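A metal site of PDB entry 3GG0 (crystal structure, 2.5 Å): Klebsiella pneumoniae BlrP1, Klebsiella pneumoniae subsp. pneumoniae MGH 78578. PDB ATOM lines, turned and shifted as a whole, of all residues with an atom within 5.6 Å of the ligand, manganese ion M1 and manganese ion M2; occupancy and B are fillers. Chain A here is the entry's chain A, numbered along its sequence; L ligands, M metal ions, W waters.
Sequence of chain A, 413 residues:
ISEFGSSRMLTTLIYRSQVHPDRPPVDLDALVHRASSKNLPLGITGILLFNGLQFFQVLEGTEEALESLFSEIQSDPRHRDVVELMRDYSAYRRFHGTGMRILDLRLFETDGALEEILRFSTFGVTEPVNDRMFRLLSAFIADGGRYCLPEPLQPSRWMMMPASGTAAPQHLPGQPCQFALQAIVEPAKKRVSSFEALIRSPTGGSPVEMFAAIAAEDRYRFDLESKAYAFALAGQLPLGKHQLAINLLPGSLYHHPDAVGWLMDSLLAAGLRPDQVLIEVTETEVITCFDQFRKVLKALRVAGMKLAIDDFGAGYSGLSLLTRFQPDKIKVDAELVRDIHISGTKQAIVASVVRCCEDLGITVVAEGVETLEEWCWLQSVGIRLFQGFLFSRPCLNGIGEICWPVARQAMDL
The backbone carbonyl oxygen (O) of Glu 280 is in hydrogen-bond range of the backbone NH (N) of Leu 248. NE2 of Gln 387 lies within hydrogen-bond range of OE1 of Glu 196 (2.7 Å). N of Leu 249 is in hydrogen-bond range of OD2 of Asp 223, at 3.1 Å. OE2 of Glu 370 is in salt-bridge range of NH2 of Arg 338 (3.1 Å). The backbone carbonyl oxygen (O) of Leu 198 sits at hydrogen-bond distance from the guanidinium group (NH1) of Arg 200, at 3.4 Å. The backbone carbonyl oxygen (O) of Gly 368 sits at hydrogen-bond distance from the guanidinium group (NH1) of Arg 338 (2.6 Å). N of Gly 368 is in hydrogen-bond range of O of Gln 387. O of Gln 387 is in hydrogen-bond range of N of Val 369 (3.3 Å).
Water W3 lies within hydrogen-bond range of NZ of Lys 331, OE1 of Glu 196 and O3 of the ligand. Water W4 lies within hydrogen-bond range of an oxygen (O14) of the ligand, the backbone carbonyl oxygen (O) of Ala 197 and the backbone NH (N) of Asn 247.
Manganese ion M2 is bound by the side-chain carboxylate (OE1) of Glu 367, the side-chain carboxylate (OD1) of Asp 311, an oxygen (O2) of the ligand, the side-chain carboxylate (OD1) of Asp 310, water W3 and the side-chain carboxylate (OE2) of Glu 367. Manganese ion M2 has six donor atoms within binding distance.
Residues that only touch the ligand: Phe 179 (3.8 Å), Leu 198 (3.3 Å), Pro 207 (3.4 Å), Leu 249 (3.5 Å), Arg 338 (3.6 Å), Gly 368 (3.4 Å), Val 369 (3.7 Å), Gly 388 (3.3 Å) and Pro 394 (3.5 Å). Hydrophobic or aromatic side chains that line the ligand: Phe 179, Leu 198, Ile 199, Pro 207, Leu 249, Phe 389 and Pro 394. The nearest printed residue that does not touch the ligand is Phe 211 (4.1 Å).
Manganese ion M1 is bound by OE2 of Glu 280, OE2 of Glu 196, OD1 of Asn 247, OD2 of Asp 310, O1 of the ligand and water W3. Manganese ion M1 has six donor atoms within binding distance.
N8 of the ligand lies within hydrogen-bond range of O of Asn 247 (3.0 Å). The backbone NH (N) of Phe 389 is in hydrogen-bond range of an oxygen (O7) of the ligand, 2.7 Å away. The side-chain carboxylate (OD1) of Asp 223 is in hydrogen-bond range of a nitrogen (N8) of the ligand (2.8 Å). The side-chain amino group (NZ) of Lys 227 is in hydrogen-bond range of an oxygen (O14) of the ligand (2.8 Å). A nitrogen (N3) of the ligand lies within hydrogen-bond range of the side-chain carboxylate (OE2) of Glu 370 (2.9 Å). The backbone NH of Ile 199 lies within hydrogen-bond range of a nitrogen (N7) of the ligand (3.0 Å). The side-chain amide nitrogen (NE2) of Gln 182 sits at hydrogen-bond distance from a nitrogen (N2) of the ligand. An oxygen (O9) of the ligand lies within salt-bridge range of the guanidinium group of Arg 200 (3.1 Å).
Three residues have an atom within 4 Å of manganese ion M2: Asp 310, Asp 311 and Glu 367.
Residues that only touch manganese ion M1: Lys 331 (3.8 Å). Of the 32 residues printed, 5 come within 4 Å of manganese ion M1. The nearest printed residue that does not touch manganese ion M1 is Glu 367 (4.8 Å).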
ATOM      1  N   PHE A 179     -16.716  -8.142 -16.903  1.00  0.00           N
ATOM      2  CA  PHE A 179     -17.675  -7.221 -17.484  1.00  0.00           C
ATOM      3  C   PHE A 179     -17.094  -6.478 -18.668  1.00  0.00           C
ATOM      4  O   PHE A 179     -15.900  -6.171 -18.706  1.00  0.00           O
ATOM      5  CB  PHE A 179     -18.175  -6.238 -16.430  1.00  0.00           C
ATOM      6  CG  PHE A 179     -19.155  -6.833 -15.459  1.00  0.00           C
ATOM      7  CD1 PHE A 179     -18.723  -7.631 -14.395  1.00  0.00           C
ATOM      8  CD2 PHE A 179     -20.526  -6.625 -15.614  1.00  0.00           C
ATOM      9  CE1 PHE A 179     -19.632  -8.186 -13.508  1.00  0.00           C
ATOM     10  CE2 PHE A 179     -21.440  -7.167 -14.727  1.00  0.00           C
ATOM     11  CZ  PHE A 179     -20.995  -7.960 -13.673  1.00  0.00           C
ATOM     12  N   GLN A 182     -20.014  -0.397 -22.003  1.00  0.00           N
ATOM     13  CA  GLN A 182     -20.471   0.404 -23.127  1.00  0.00           C
ATOM     14  C   GLN A 182     -20.789   1.818 -22.686  1.00  0.00           C
ATOM     15  O   GLN A 182     -21.476   2.028 -21.682  1.00  0.00           O
ATOM     16  CB  GLN A 182     -21.695  -0.235 -23.786  1.00  0.00           C
ATOM     17  CG  GLN A 182     -22.086   0.437 -25.106  1.00  0.00           C
ATOM     18  CD  GLN A 182     -23.233  -0.263 -25.800  1.00  0.00           C
ATOM     19  OE1 GLN A 182     -23.998  -1.012 -25.181  1.00  0.00           O
ATOM     20  NE2 GLN A 182     -23.379  -0.016 -27.093  1.00  0.00           N
ATOM     21  N   GLU A 196     -22.306   1.509 -19.130  1.00  0.00           N
ATOM     22  CA  GLU A 196     -23.062   0.345 -18.676  1.00  0.00           C
ATOM     23  C   GLU A 196     -22.160  -0.872 -18.585  1.00  0.00           C
ATOM     24  O   GLU A 196     -21.444  -1.197 -19.526  1.00  0.00           O
ATOM     25  CB  GLU A 196     -24.246   0.055 -19.608  1.00  0.00           C
ATOM     26  CG  GLU A 196     -25.300  -0.875 -18.967  1.00  0.00           C
ATOM     27  CD  GLU A 196     -26.378  -1.334 -19.942  1.00  0.00           C
ATOM     28  OE1 GLU A 196     -26.524  -0.732 -21.034  1.00  0.00           O
ATOM     29  OE2 GLU A 196     -27.083  -2.306 -19.605  1.00  0.00           O
ATOM     30  N   ALA A 197     -22.193  -1.536 -17.428  1.00  0.00           N
ATOM     31  CA  ALA A 197     -21.490  -2.787 -17.235  1.00  0.00           C
ATOM     32  C   ALA A 197     -22.337  -3.949 -17.729  1.00  0.00           C
ATOM     33  O   ALA A 197     -23.491  -4.093 -17.318  1.00  0.00           O
ATOM     34  CB  ALA A 197     -21.133  -2.967 -15.781  1.00  0.00           C
ATOM     35  N   LEU A 198     -21.765  -4.767 -18.600  1.00  0.00           N
ATOM     36  CA  LEU A 198     -22.469  -5.910 -19.177  1.00  0.00           C
ATOM     37  C   LEU A 198     -21.695  -7.193 -18.903  1.00  0.00           C
ATOM     38  O   LEU A 198     -20.547  -7.343 -19.329  1.00  0.00           O
ATOM     39  CB  LEU A 198     -22.646  -5.720 -20.683  1.00  0.00           C
ATOM     40  CG  LEU A 198     -23.402  -4.470 -21.144  1.00  0.00           C
ATOM     41  CD1 LEU A 198     -23.154  -4.189 -22.619  1.00  0.00           C
ATOM     42  CD2 LEU A 198     -24.880  -4.588 -20.849  1.00  0.00           C
ATOM     43  N   ILE A 199     -22.328  -8.126 -18.190  1.00  0.00           N
ATOM     44  CA  ILE A 199     -21.653  -9.332 -17.699  1.00  0.00           C
ATOM     45  C   ILE A 199     -21.149 -10.248 -18.830  1.00  0.00           C
ATOM     46  O   ILE A 199     -21.832 -10.472 -19.833  1.00  0.00           O
ATOM     47  CB  ILE A 199     -22.551 -10.116 -16.715  1.00  0.00           C
ATOM     48  CG1 ILE A 199     -21.704 -11.073 -15.866  1.00  0.00           C
ATOM     49  CG2 ILE A 199     -23.663 -10.854 -17.442  1.00  0.00           C
ATOM     50  CD1 ILE A 199     -22.441 -11.655 -14.676  1.00  0.00           C
ATOM     51  N   ARG A 200     -19.927 -10.744 -18.668  1.00  0.00           N
ATOM     52  CA  ARG A 200     -19.354 -11.709 -19.594  1.00  0.00           C
ATOM     53  C   ARG A 200     -18.845 -12.931 -18.855  1.00  0.00           C
ATOM     54  O   ARG A 200     -18.415 -12.840 -17.693  1.00  0.00           O
ATOM     55  CB  ARG A 200     -18.210 -11.074 -20.401  1.00  0.00           C
ATOM     56  CG  ARG A 200     -18.616  -9.846 -21.221  1.00  0.00           C
ATOM     57  CD  ARG A 200     -19.377 -10.247 -22.470  1.00  0.00           C
ATOM     58  NE  ARG A 200     -19.736  -9.093 -23.290  1.00  0.00           N
ATOM     59  CZ  ARG A 200     -20.868  -8.412 -23.149  1.00  0.00           C
ATOM     60  NH1 ARG A 200     -21.763  -8.754 -22.223  1.00  0.00           N
ATOM     61  NH2 ARG A 200     -21.119  -7.371 -23.943  1.00  0.00           N
ATOM     62  N   SER A 206     -21.097 -14.544 -23.733  1.00  0.00           N
ATOM     63  CA  SER A 206     -22.288 -13.723 -23.526  1.00  0.00           C
ATOM     64  C   SER A 206     -22.874 -13.859 -22.113  1.00  0.00           C
ATOM     65  O   SER A 206     -22.558 -14.810 -21.405  1.00  0.00           O
ATOM     66  CB  SER A 206     -23.354 -14.083 -24.570  1.00  0.00           C
ATOM     67  OG  SER A 206     -24.009 -15.284 -24.250  1.00  0.00           O
ATOM     68  N   PRO A 207     -23.710 -12.886 -21.699  1.00  0.00           N
ATOM     69  CA  PRO A 207     -24.512 -12.989 -20.468  1.00  0.00           C
ATOM     70  C   PRO A 207     -25.243 -14.325 -20.341  1.00  0.00           C
ATOM     71  O   PRO A 207     -25.268 -14.913 -19.250  1.00  0.00           O
ATOM     72  CB  PRO A 207     -25.523 -11.845 -20.624  1.00  0.00           C
ATOM     73  CG  PRO A 207     -24.792 -10.825 -21.414  1.00  0.00           C
ATOM     74  CD  PRO A 207     -23.904 -11.584 -22.365  1.00  0.00           C
ATOM     75  N   PHE A 211     -24.719 -17.122 -17.313  1.00  0.00           N
ATOM     76  CA  PHE A 211     -25.764 -17.593 -16.406  1.00  0.00           C
ATOM     77  C   PHE A 211     -26.114 -19.069 -16.613  1.00  0.00           C
ATOM     78  O   PHE A 211     -26.593 -19.720 -15.690  1.00  0.00           O
ATOM     79  CB  PHE A 211     -27.012 -16.711 -16.517  1.00  0.00           C
ATOM     80  CG  PHE A 211     -26.941 -15.445 -15.701  1.00  0.00           C
ATOM     81  CD1 PHE A 211     -27.142 -15.468 -14.326  1.00  0.00           C
ATOM     82  CD2 PHE A 211     -26.659 -14.223 -16.316  1.00  0.00           C
ATOM     83  CE1 PHE A 211     -27.066 -14.309 -13.580  1.00  0.00           C
ATOM     84  CE2 PHE A 211     -26.584 -13.056 -15.576  1.00  0.00           C
ATOM     85  CZ  PHE A 211     -26.790 -13.096 -14.204  1.00  0.00           C
ATOM     86  N   ASP A 223     -26.095 -13.059  -9.732  1.00  0.00           N
ATOM     87  CA  ASP A 223     -26.368 -11.773 -10.379  1.00  0.00           C
ATOM     88  C   ASP A 223     -26.011 -10.614  -9.450  1.00  0.00           C
ATOM     89  O   ASP A 223     -25.377  -9.648  -9.867  1.00  0.00           O
ATOM     90  CB  ASP A 223     -27.842 -11.682 -10.799  1.00  0.00           C
ATOM     91  CG  ASP A 223     -28.169 -10.401 -11.544  1.00  0.00           C
ATOM     92  OD1 ASP A 223     -27.267  -9.834 -12.192  1.00  0.00           O
ATOM     93  OD2 ASP A 223     -29.335  -9.960 -11.490  1.00  0.00           O
ATOM     94  N   SER A 226     -21.996 -10.787  -8.592  1.00  0.00           N
ATOM     95  CA  SER A 226     -21.120 -10.393  -9.709  1.00  0.00           C
ATOM     96  C   SER A 226     -20.917  -8.888  -9.821  1.00  0.00           C
ATOM     97  O   SER A 226     -19.911  -8.442 -10.356  1.00  0.00           O
ATOM     98  CB  SER A 226     -21.648 -10.954 -11.031  1.00  0.00           C
ATOM     99  OG  SER A 226     -22.956 -10.481 -11.310  1.00  0.00           O
ATOM    100  N   LYS A 227     -21.857  -8.120  -9.284  1.00  0.00           N
ATOM    101  CA  LYS A 227     -21.779  -6.664  -9.335  1.00  0.00           C
ATOM    102  C   LYS A 227     -20.556  -6.103  -8.629  1.00  0.00           C
ATOM    103  O   LYS A 227     -20.096  -5.010  -8.955  1.00  0.00           O
ATOM    104  CB  LYS A 227     -23.062  -6.045  -8.749  1.00  0.00           C
ATOM    105  CG  LYS A 227     -24.293  -6.274  -9.601  1.00  0.00           C
ATOM    106  CD  LYS A 227     -23.945  -6.229 -11.073  1.00  0.00           C
ATOM    107  CE  LYS A 227     -25.139  -6.497 -11.930  1.00  0.00           C
ATOM    108  NZ  LYS A 227     -25.364  -7.951 -12.135  1.00  0.00           N
ATOM    109  N   ASN A 247     -27.123  -3.804 -14.536  1.00  0.00           N
ATOM    110  CA  ASN A 247     -28.338  -4.592 -14.742  1.00  0.00           C
ATOM    111  C   ASN A 247     -28.569  -5.589 -13.614  1.00  0.00           C
ATOM    112  O   ASN A 247     -27.763  -6.488 -13.392  1.00  0.00           O
ATOM    113  CB  ASN A 247     -28.274  -5.344 -16.080  1.00  0.00           C
ATOM    114  CG  ASN A 247     -28.084  -4.425 -17.269  1.00  0.00           C
ATOM    115  OD1 ASN A 247     -29.058  -3.996 -17.901  1.00  0.00           O
ATOM    116  ND2 ASN A 247     -26.822  -4.135 -17.588  1.00  0.00           N
ATOM    117  N   LEU A 248     -29.648  -5.435 -12.871  1.00  0.00           N
ATOM    118  CA  LEU A 248     -30.070  -6.438 -11.895  1.00  0.00           C
ATOM    119  C   LEU A 248     -31.513  -6.846 -12.138  1.00  0.00           C
ATOM    120  O   LEU A 248     -32.372  -5.989 -12.359  1.00  0.00           O
ATOM    121  CB  LEU A 248     -29.908  -5.920 -10.467  1.00  0.00           C
ATOM    122  CG  LEU A 248     -28.523  -5.967  -9.826  1.00  0.00           C
ATOM    123  CD1 LEU A 248     -28.552  -5.279  -8.460  1.00  0.00           C
ATOM    124  CD2 LEU A 248     -28.030  -7.387  -9.698  1.00  0.00           C
ATOM    125  N   LEU A 249     -31.775  -8.142 -12.096  1.00  0.00           N
ATOM    126  CA  LEU A 249     -33.136  -8.641 -11.997  1.00  0.00           C
ATOM    127  C   LEU A 249     -33.683  -8.308 -10.613  1.00  0.00           C
ATOM    128  O   LEU A 249     -32.944  -8.365  -9.626  1.00  0.00           O
ATOM    129  CB  LEU A 249     -33.182 -10.156 -12.244  1.00  0.00           C
ATOM    130  CG  LEU A 249     -32.522 -10.658 -13.529  1.00  0.00           C
ATOM    131  CD1 LEU A 249     -32.583 -12.181 -13.626  1.00  0.00           C
ATOM    132  CD2 LEU A 249     -33.142 -10.014 -14.769  1.00  0.00           C
ATOM    133  N   GLU A 280     -30.210  -0.810 -13.389  1.00  0.00           N
ATOM    134  CA  GLU A 280     -31.092  -1.029 -14.529  1.00  0.00           C
ATOM    135  C   GLU A 280     -31.956  -2.261 -14.311  1.00  0.00           C
ATOM    136  O   GLU A 280     -31.460  -3.383 -14.228  1.00  0.00           O
ATOM    137  CB  GLU A 280     -30.280  -1.206 -15.805  1.00  0.00           C
ATOM    138  CG  GLU A 280     -29.595   0.048 -16.301  1.00  0.00           C
ATOM    139  CD  GLU A 280     -29.017  -0.115 -17.685  1.00  0.00           C
ATOM    140  OE1 GLU A 280     -28.168   0.716 -18.079  1.00  0.00           O
ATOM    141  OE2 GLU A 280     -29.410  -1.061 -18.394  1.00  0.00           O
ATOM    142  N   THR A 282     -35.347  -4.397 -15.914  1.00  0.00           N
ATOM    143  CA  THR A 282     -36.140  -4.571 -17.133  1.00  0.00           C
ATOM    144  C   THR A 282     -37.619  -4.308 -16.892  1.00  0.00           C
ATOM    145  O   THR A 282     -38.185  -4.726 -15.879  1.00  0.00           O
ATOM    146  CB  THR A 282     -35.966  -5.964 -17.759  1.00  0.00           C
ATOM    147  OG1 THR A 282     -35.755  -6.931 -16.726  1.00  0.00           O
ATOM    148  CG2 THR A 282     -34.789  -5.978 -18.704  1.00  0.00           C
ATOM    149  N   ASP A 310     -34.886  -0.307 -17.739  1.00  0.00           N
ATOM    150  CA  ASP A 310     -34.233  -0.780 -18.939  1.00  0.00           C
ATOM    151  C   ASP A 310     -35.242  -1.326 -19.932  1.00  0.00           C
ATOM    152  O   ASP A 310     -36.269  -1.890 -19.541  1.00  0.00           O
ATOM    153  CB  ASP A 310     -33.201  -1.847 -18.592  1.00  0.00           C
ATOM    154  CG  ASP A 310     -32.174  -2.040 -19.699  1.00  0.00           C
ATOM    155  OD1 ASP A 310     -32.176  -1.258 -20.676  1.00  0.00           O
ATOM    156  OD2 ASP A 310     -31.358  -2.974 -19.570  1.00  0.00           O
ATOM    157  N   ASP A 311     -34.955  -1.150 -21.220  1.00  0.00           N
ATOM    158  CA  ASP A 311     -35.790  -1.694 -22.305  1.00  0.00           C
ATOM    159  C   ASP A 311     -37.254  -1.250 -22.224  1.00  0.00           C
ATOM    160  O   ASP A 311     -38.172  -2.052 -22.409  1.00  0.00           O
ATOM    161  CB  ASP A 311     -35.674  -3.223 -22.361  1.00  0.00           C
ATOM    162  CG  ASP A 311     -34.253  -3.688 -22.689  1.00  0.00           C
ATOM    163  OD1 ASP A 311     -33.439  -2.864 -23.170  1.00  0.00           O
ATOM    164  OD2 ASP A 311     -33.954  -4.884 -22.474  1.00  0.00           O
ATOM    165  N   LYS A 331     -34.655   3.959 -20.507  1.00  0.00           N
ATOM    166  CA  LYS A 331     -33.922   3.545 -21.704  1.00  0.00           C
ATOM    167  C   LYS A 331     -34.871   3.002 -22.747  1.00  0.00           C
ATOM    168  O   LYS A 331     -35.412   1.907 -22.608  1.00  0.00           O
ATOM    169  CB  LYS A 331     -32.847   2.525 -21.368  1.00  0.00           C
ATOM    170  CG  LYS A 331     -31.867   2.972 -20.288  1.00  0.00           C
ATOM    171  CD  LYS A 331     -30.829   1.911 -19.999  1.00  0.00           C
ATOM    172  CE  LYS A 331     -29.603   2.111 -20.842  1.00  0.00           C
ATOM    173  NZ  LYS A 331     -28.737   0.903 -20.849  1.00  0.00           N
ATOM    174  N   ARG A 338     -34.991   0.887 -34.122  1.00  0.00           N
ATOM    175  CA  ARG A 338     -34.917   0.250 -35.444  1.00  0.00           C
ATOM    176  C   ARG A 338     -35.877   0.895 -36.400  1.00  0.00           C
ATOM    177  O   ARG A 338     -37.093   0.862 -36.180  1.00  0.00           O
ATOM    178  CB  ARG A 338     -35.238  -1.244 -35.356  1.00  0.00           C
ATOM    179  CG  ARG A 338     -34.128  -2.098 -34.833  1.00  0.00           C
ATOM    180  CD  ARG A 338     -32.868  -2.035 -35.704  1.00  0.00           C
ATOM    181  NE  ARG A 338     -31.708  -2.422 -34.909  1.00  0.00           N
ATOM    182  CZ  ARG A 338     -30.988  -1.587 -34.172  1.00  0.00           C
ATOM    183  NH1 ARG A 338     -31.275  -0.289 -34.166  1.00  0.00           N
ATOM    184  NH2 ARG A 338     -29.982  -2.041 -33.446  1.00  0.00           N
ATOM    185  N   GLU A 367     -31.572   3.362 -27.200  1.00  0.00           N
ATOM    186  CA  GLU A 367     -30.711   2.183 -27.219  1.00  0.00           C
ATOM    187  C   GLU A 367     -30.609   1.583 -28.594  1.00  0.00           C
ATOM    188  O   GLU A 367     -31.496   1.748 -29.417  1.00  0.00           O
ATOM    189  CB  GLU A 367     -31.260   1.137 -26.285  1.00  0.00           C
ATOM    190  CG  GLU A 367     -30.562   1.022 -24.986  1.00  0.00           C
ATOM    191  CD  GLU A 367     -31.096  -0.108 -24.174  1.00  0.00           C
ATOM    192  OE1 GLU A 367     -30.358  -1.086 -23.932  1.00  0.00           O
ATOM    193  OE2 GLU A 367     -32.290  -0.052 -23.814  1.00  0.00           O
ATOM    194  N   GLY A 368     -29.525   0.839 -28.826  1.00  0.00           N
ATOM    195  CA  GLY A 368     -29.353   0.088 -30.059  1.00  0.00           C
ATOM    196  C   GLY A 368     -29.249   0.971 -31.286  1.00  0.00           C
ATOM    197  O   GLY A 368     -29.613   0.552 -32.381  1.00  0.00           O
ATOM    198  N   VAL A 369     -28.745   2.188 -31.109  1.00  0.00           N
ATOM    199  CA  VAL A 369     -28.530   3.119 -32.223  1.00  0.00           C
ATOM    200  C   VAL A 369     -27.346   2.680 -33.089  1.00  0.00           C
ATOM    201  O   VAL A 369     -26.199   2.672 -32.635  1.00  0.00           O
ATOM    202  CB  VAL A 369     -28.299   4.562 -31.727  1.00  0.00           C
ATOM    203  CG1 VAL A 369     -28.226   5.521 -32.906  1.00  0.00           C
ATOM    204  CG2 VAL A 369     -29.407   4.978 -30.769  1.00  0.00           C
ATOM    205  N   GLU A 370     -27.633   2.314 -34.333  1.00  0.00           N
ATOM    206  CA  GLU A 370     -26.624   1.707 -35.202  1.00  0.00           C
ATOM    207  C   GLU A 370     -26.290   2.559 -36.423  1.00  0.00           C
ATOM    208  O   GLU A 370     -25.235   2.380 -37.036  1.00  0.00           O
ATOM    209  CB  GLU A 370     -27.087   0.327 -35.663  1.00  0.00           C
ATOM    210  CG  GLU A 370     -27.018  -0.746 -34.591  1.00  0.00           C
ATOM    211  CD  GLU A 370     -27.552  -2.081 -35.086  1.00  0.00           C
ATOM    212  OE1 GLU A 370     -28.272  -2.092 -36.093  1.00  0.00           O
ATOM    213  OE2 GLU A 370     -27.254  -3.110 -34.441  1.00  0.00           O
ATOM    214  N   GLN A 387     -27.093   5.356 -26.805  1.00  0.00           N
ATOM    215  CA  GLN A 387     -26.288   4.171 -26.587  1.00  0.00           C
ATOM    216  C   GLN A 387     -26.423   3.239 -27.780  1.00  0.00           C
ATOM    217  O   GLN A 387     -27.533   2.863 -28.155  1.00  0.00           O
ATOM    218  CB  GLN A 387     -26.721   3.452 -25.305  1.00  0.00           C
ATOM    219  CG  GLN A 387     -25.959   2.155 -25.014  1.00  0.00           C
ATOM    220  CD  GLN A 387     -26.325   1.540 -23.674  1.00  0.00           C
ATOM    221  OE1 GLN A 387     -27.250   1.965 -23.005  1.00  0.00           O
ATOM    222  NE2 GLN A 387     -25.592   0.519 -23.277  1.00  0.00           N
ATOM    223  N   GLY A 388     -25.305   2.872 -28.393  1.00  0.00           N
ATOM    224  CA  GLY A 388     -25.334   1.951 -29.517  1.00  0.00           C
ATOM    225  C   GLY A 388     -24.012   1.707 -30.200  1.00  0.00           C
ATOM    226  O   GLY A 388     -23.030   2.423 -29.952  1.00  0.00           O
ATOM    227  N   PHE A 389     -23.986   0.699 -31.070  1.00  0.00           N
ATOM    228  CA  PHE A 389     -22.768   0.299 -31.779  1.00  0.00           C
ATOM    229  C   PHE A 389     -22.229   1.407 -32.683  1.00  0.00           C
ATOM    230  O   PHE A 389     -21.040   1.422 -33.002  1.00  0.00           O
ATOM    231  CB  PHE A 389     -23.025  -0.958 -32.615  1.00  0.00           C
ATOM    232  CG  PHE A 389     -23.206  -2.209 -31.807  1.00  0.00           C
ATOM    233  CD1 PHE A 389     -22.858  -2.250 -30.466  1.00  0.00           C
ATOM    234  CD2 PHE A 389     -23.713  -3.362 -32.398  1.00  0.00           C
ATOM    235  CE1 PHE A 389     -23.017  -3.414 -29.711  1.00  0.00           C
ATOM    236  CE2 PHE A 389     -23.864  -4.537 -31.657  1.00  0.00           C
ATOM    237  CZ  PHE A 389     -23.525  -4.552 -30.315  1.00  0.00           C
ATOM    238  N   LEU A 390     -23.112   2.329 -33.094  1.00  0.00           N
ATOM    239  CA  LEU A 390     -22.708   3.486 -33.878  1.00  0.00           C
ATOM    240  C   LEU A 390     -21.679   4.328 -33.142  1.00  0.00           C
ATOM    241  O   LEU A 390     -20.679   4.745 -33.728  1.00  0.00           O
ATOM    242  CB  LEU A 390     -23.918   4.338 -34.236  1.00  0.00           C
ATOM    243  CG  LEU A 390     -23.640   5.582 -35.093  1.00  0.00           C
ATOM    244  CD1 LEU A 390     -23.332   5.197 -36.538  1.00  0.00           C
ATOM    245  CD2 LEU A 390     -24.802   6.559 -35.029  1.00  0.00           C
ATOM    246  N   SER A 392     -20.305   3.465 -29.778  1.00  0.00           N
ATOM    247  CA  SER A 392     -19.413   2.747 -28.876  1.00  0.00           C
ATOM    248  C   SER A 392     -19.834   1.302 -28.704  1.00  0.00           C
ATOM    249  O   SER A 392     -20.984   1.007 -28.384  1.00  0.00           O
ATOM    250  CB  SER A 392     -19.379   3.442 -27.506  1.00  0.00           C
ATOM    251  OG  SER A 392     -18.597   2.719 -26.569  1.00  0.00           O
ATOM    252  N   PRO A 394     -19.360  -2.454 -26.701  1.00  0.00           N
ATOM    253  CA  PRO A 394     -18.924  -3.096 -25.475  1.00  0.00           C
ATOM    254  C   PRO A 394     -17.456  -3.458 -25.519  1.00  0.00           C
ATOM    255  O   PRO A 394     -16.989  -4.059 -26.495  1.00  0.00           O
ATOM    256  CB  PRO A 394     -19.774  -4.363 -25.429  1.00  0.00           C
ATOM    257  CG  PRO A 394     -21.026  -3.987 -26.103  1.00  0.00           C
ATOM    258  CD  PRO A 394     -20.644  -2.999 -27.176  1.00  0.00           C
HETATM  259  P1  LIG L   1     -29.398  -4.837 -22.060  1.00  0.00           P
HETATM  260  O1  LIG L   1     -28.639  -4.497 -20.808  1.00  0.00           O
HETATM  261  O2  LIG L   1     -30.841  -4.439 -21.861  1.00  0.00           O
HETATM  262  O3  LIG L   1     -28.782  -3.996 -23.285  1.00  0.00           O
HETATM  263  C1  LIG L   1     -27.392  -4.103 -23.613  1.00  0.00           C
HETATM  264  C2  LIG L   1     -27.222  -5.117 -24.742  1.00  0.00           C
HETATM  265  O4  LIG L   1     -27.497  -4.498 -25.994  1.00  0.00           O
HETATM  266  C3  LIG L   1     -25.778  -5.558 -24.866  1.00  0.00           C
HETATM  267  O5  LIG L   1     -25.774  -6.922 -25.283  1.00  0.00           O
HETATM  268  C4  LIG L   1     -25.255  -4.734 -25.994  1.00  0.00           C
HETATM  269  O6  LIG L   1     -24.250  -5.362 -26.600  1.00  0.00           O
HETATM  270  C5  LIG L   1     -26.298  -4.596 -26.820  1.00  0.00           C
HETATM  271  N1  LIG L   1     -26.185  -3.511 -27.654  1.00  0.00           N
HETATM  272  C6  LIG L   1     -25.738  -2.371 -27.298  1.00  0.00           C
HETATM  273  N2  LIG L   1     -25.764  -1.594 -28.327  1.00  0.00           N
HETATM  274  C7  LIG L   1     -26.255  -2.249 -29.401  1.00  0.00           C
HETATM  275  C8  LIG L   1     -26.499  -1.929 -30.740  1.00  0.00           C
HETATM  276  O7  LIG L   1     -26.270  -0.783 -31.188  1.00  0.00           O
HETATM  277  N3  LIG L   1     -27.013  -2.882 -31.544  1.00  0.00           N
HETATM  278  C9  LIG L   1     -27.278  -4.132 -31.079  1.00  0.00           C
HETATM  279  N4  LIG L   1     -27.791  -5.052 -31.922  1.00  0.00           N
HETATM  280  N5  LIG L   1     -27.041  -4.459 -29.781  1.00  0.00           N
HETATM  281  C10 LIG L   1     -26.538  -3.535 -28.947  1.00  0.00           C
HETATM  282  P2  LIG L   1     -25.383  -7.925 -24.086  1.00  0.00           P
HETATM  283  O8  LIG L   1     -24.682  -9.220 -24.697  1.00  0.00           O
HETATM  284  O9  LIG L   1     -24.323  -7.270 -23.090  1.00  0.00           O
HETATM  285  O10 LIG L   1     -26.610  -8.100 -23.068  1.00  0.00           O
HETATM  286  C11 LIG L   1     -27.604  -9.115 -23.176  1.00  0.00           C
HETATM  287  C12 LIG L   1     -28.492  -8.665 -22.017  1.00  0.00           C
HETATM  288  O11 LIG L   1     -28.127  -9.347 -20.803  1.00  0.00           O
HETATM  289  C13 LIG L   1     -28.400  -7.178 -21.679  1.00  0.00           C
HETATM  290  O12 LIG L   1     -29.375  -6.426 -22.405  1.00  0.00           O
HETATM  291  C14 LIG L   1     -28.673  -7.189 -20.203  1.00  0.00           C
HETATM  292  O13 LIG L   1     -29.971  -7.378 -20.010  1.00  0.00           O
HETATM  293  C15 LIG L   1     -28.047  -8.291 -19.835  1.00  0.00           C
HETATM  294  N6  LIG L   1     -27.138  -8.266 -18.809  1.00  0.00           N
HETATM  295  C16 LIG L   1     -25.925  -7.761 -19.001  1.00  0.00           C
HETATM  296  N7  LIG L   1     -25.327  -7.823 -17.788  1.00  0.00           N
HETATM  297  C17 LIG L   1     -26.229  -8.316 -16.889  1.00  0.00           C
HETATM  298  C18 LIG L   1     -26.142  -8.581 -15.533  1.00  0.00           C
HETATM  299  O14 LIG L   1     -25.093  -8.342 -14.908  1.00  0.00           O
HETATM  300  N8  LIG L   1     -27.231  -9.079 -14.896  1.00  0.00           N
HETATM  301  C19 LIG L   1     -28.380  -9.336 -15.567  1.00  0.00           C
HETATM  302  N9  LIG L   1     -29.435  -9.847 -14.885  1.00  0.00           N
HETATM  303  N10 LIG L   1     -28.479  -9.092 -16.899  1.00  0.00           N
HETATM  304  C20 LIG L   1     -27.410  -8.577 -17.562  1.00  0.00           C
HETATM  305 MN    MN M   1     -29.186  -2.648 -19.568  1.00  0.00          MN
HETATM  306 MN    MN M   2     -31.370  -2.285 -22.656  1.00  0.00          MN
HETATM  307  O   HOH W   1     -29.429  -2.986 -27.372  1.00  0.00           O
HETATM  308  O   HOH W   2     -23.349 -11.223 -26.144  1.00  0.00           O
HETATM  309  O   HOH W   3     -29.446  -1.408 -21.551  1.00  0.00           O
HETATM  310  O   HOH W   4     -24.397  -5.799 -15.353  1.00  0.00           O
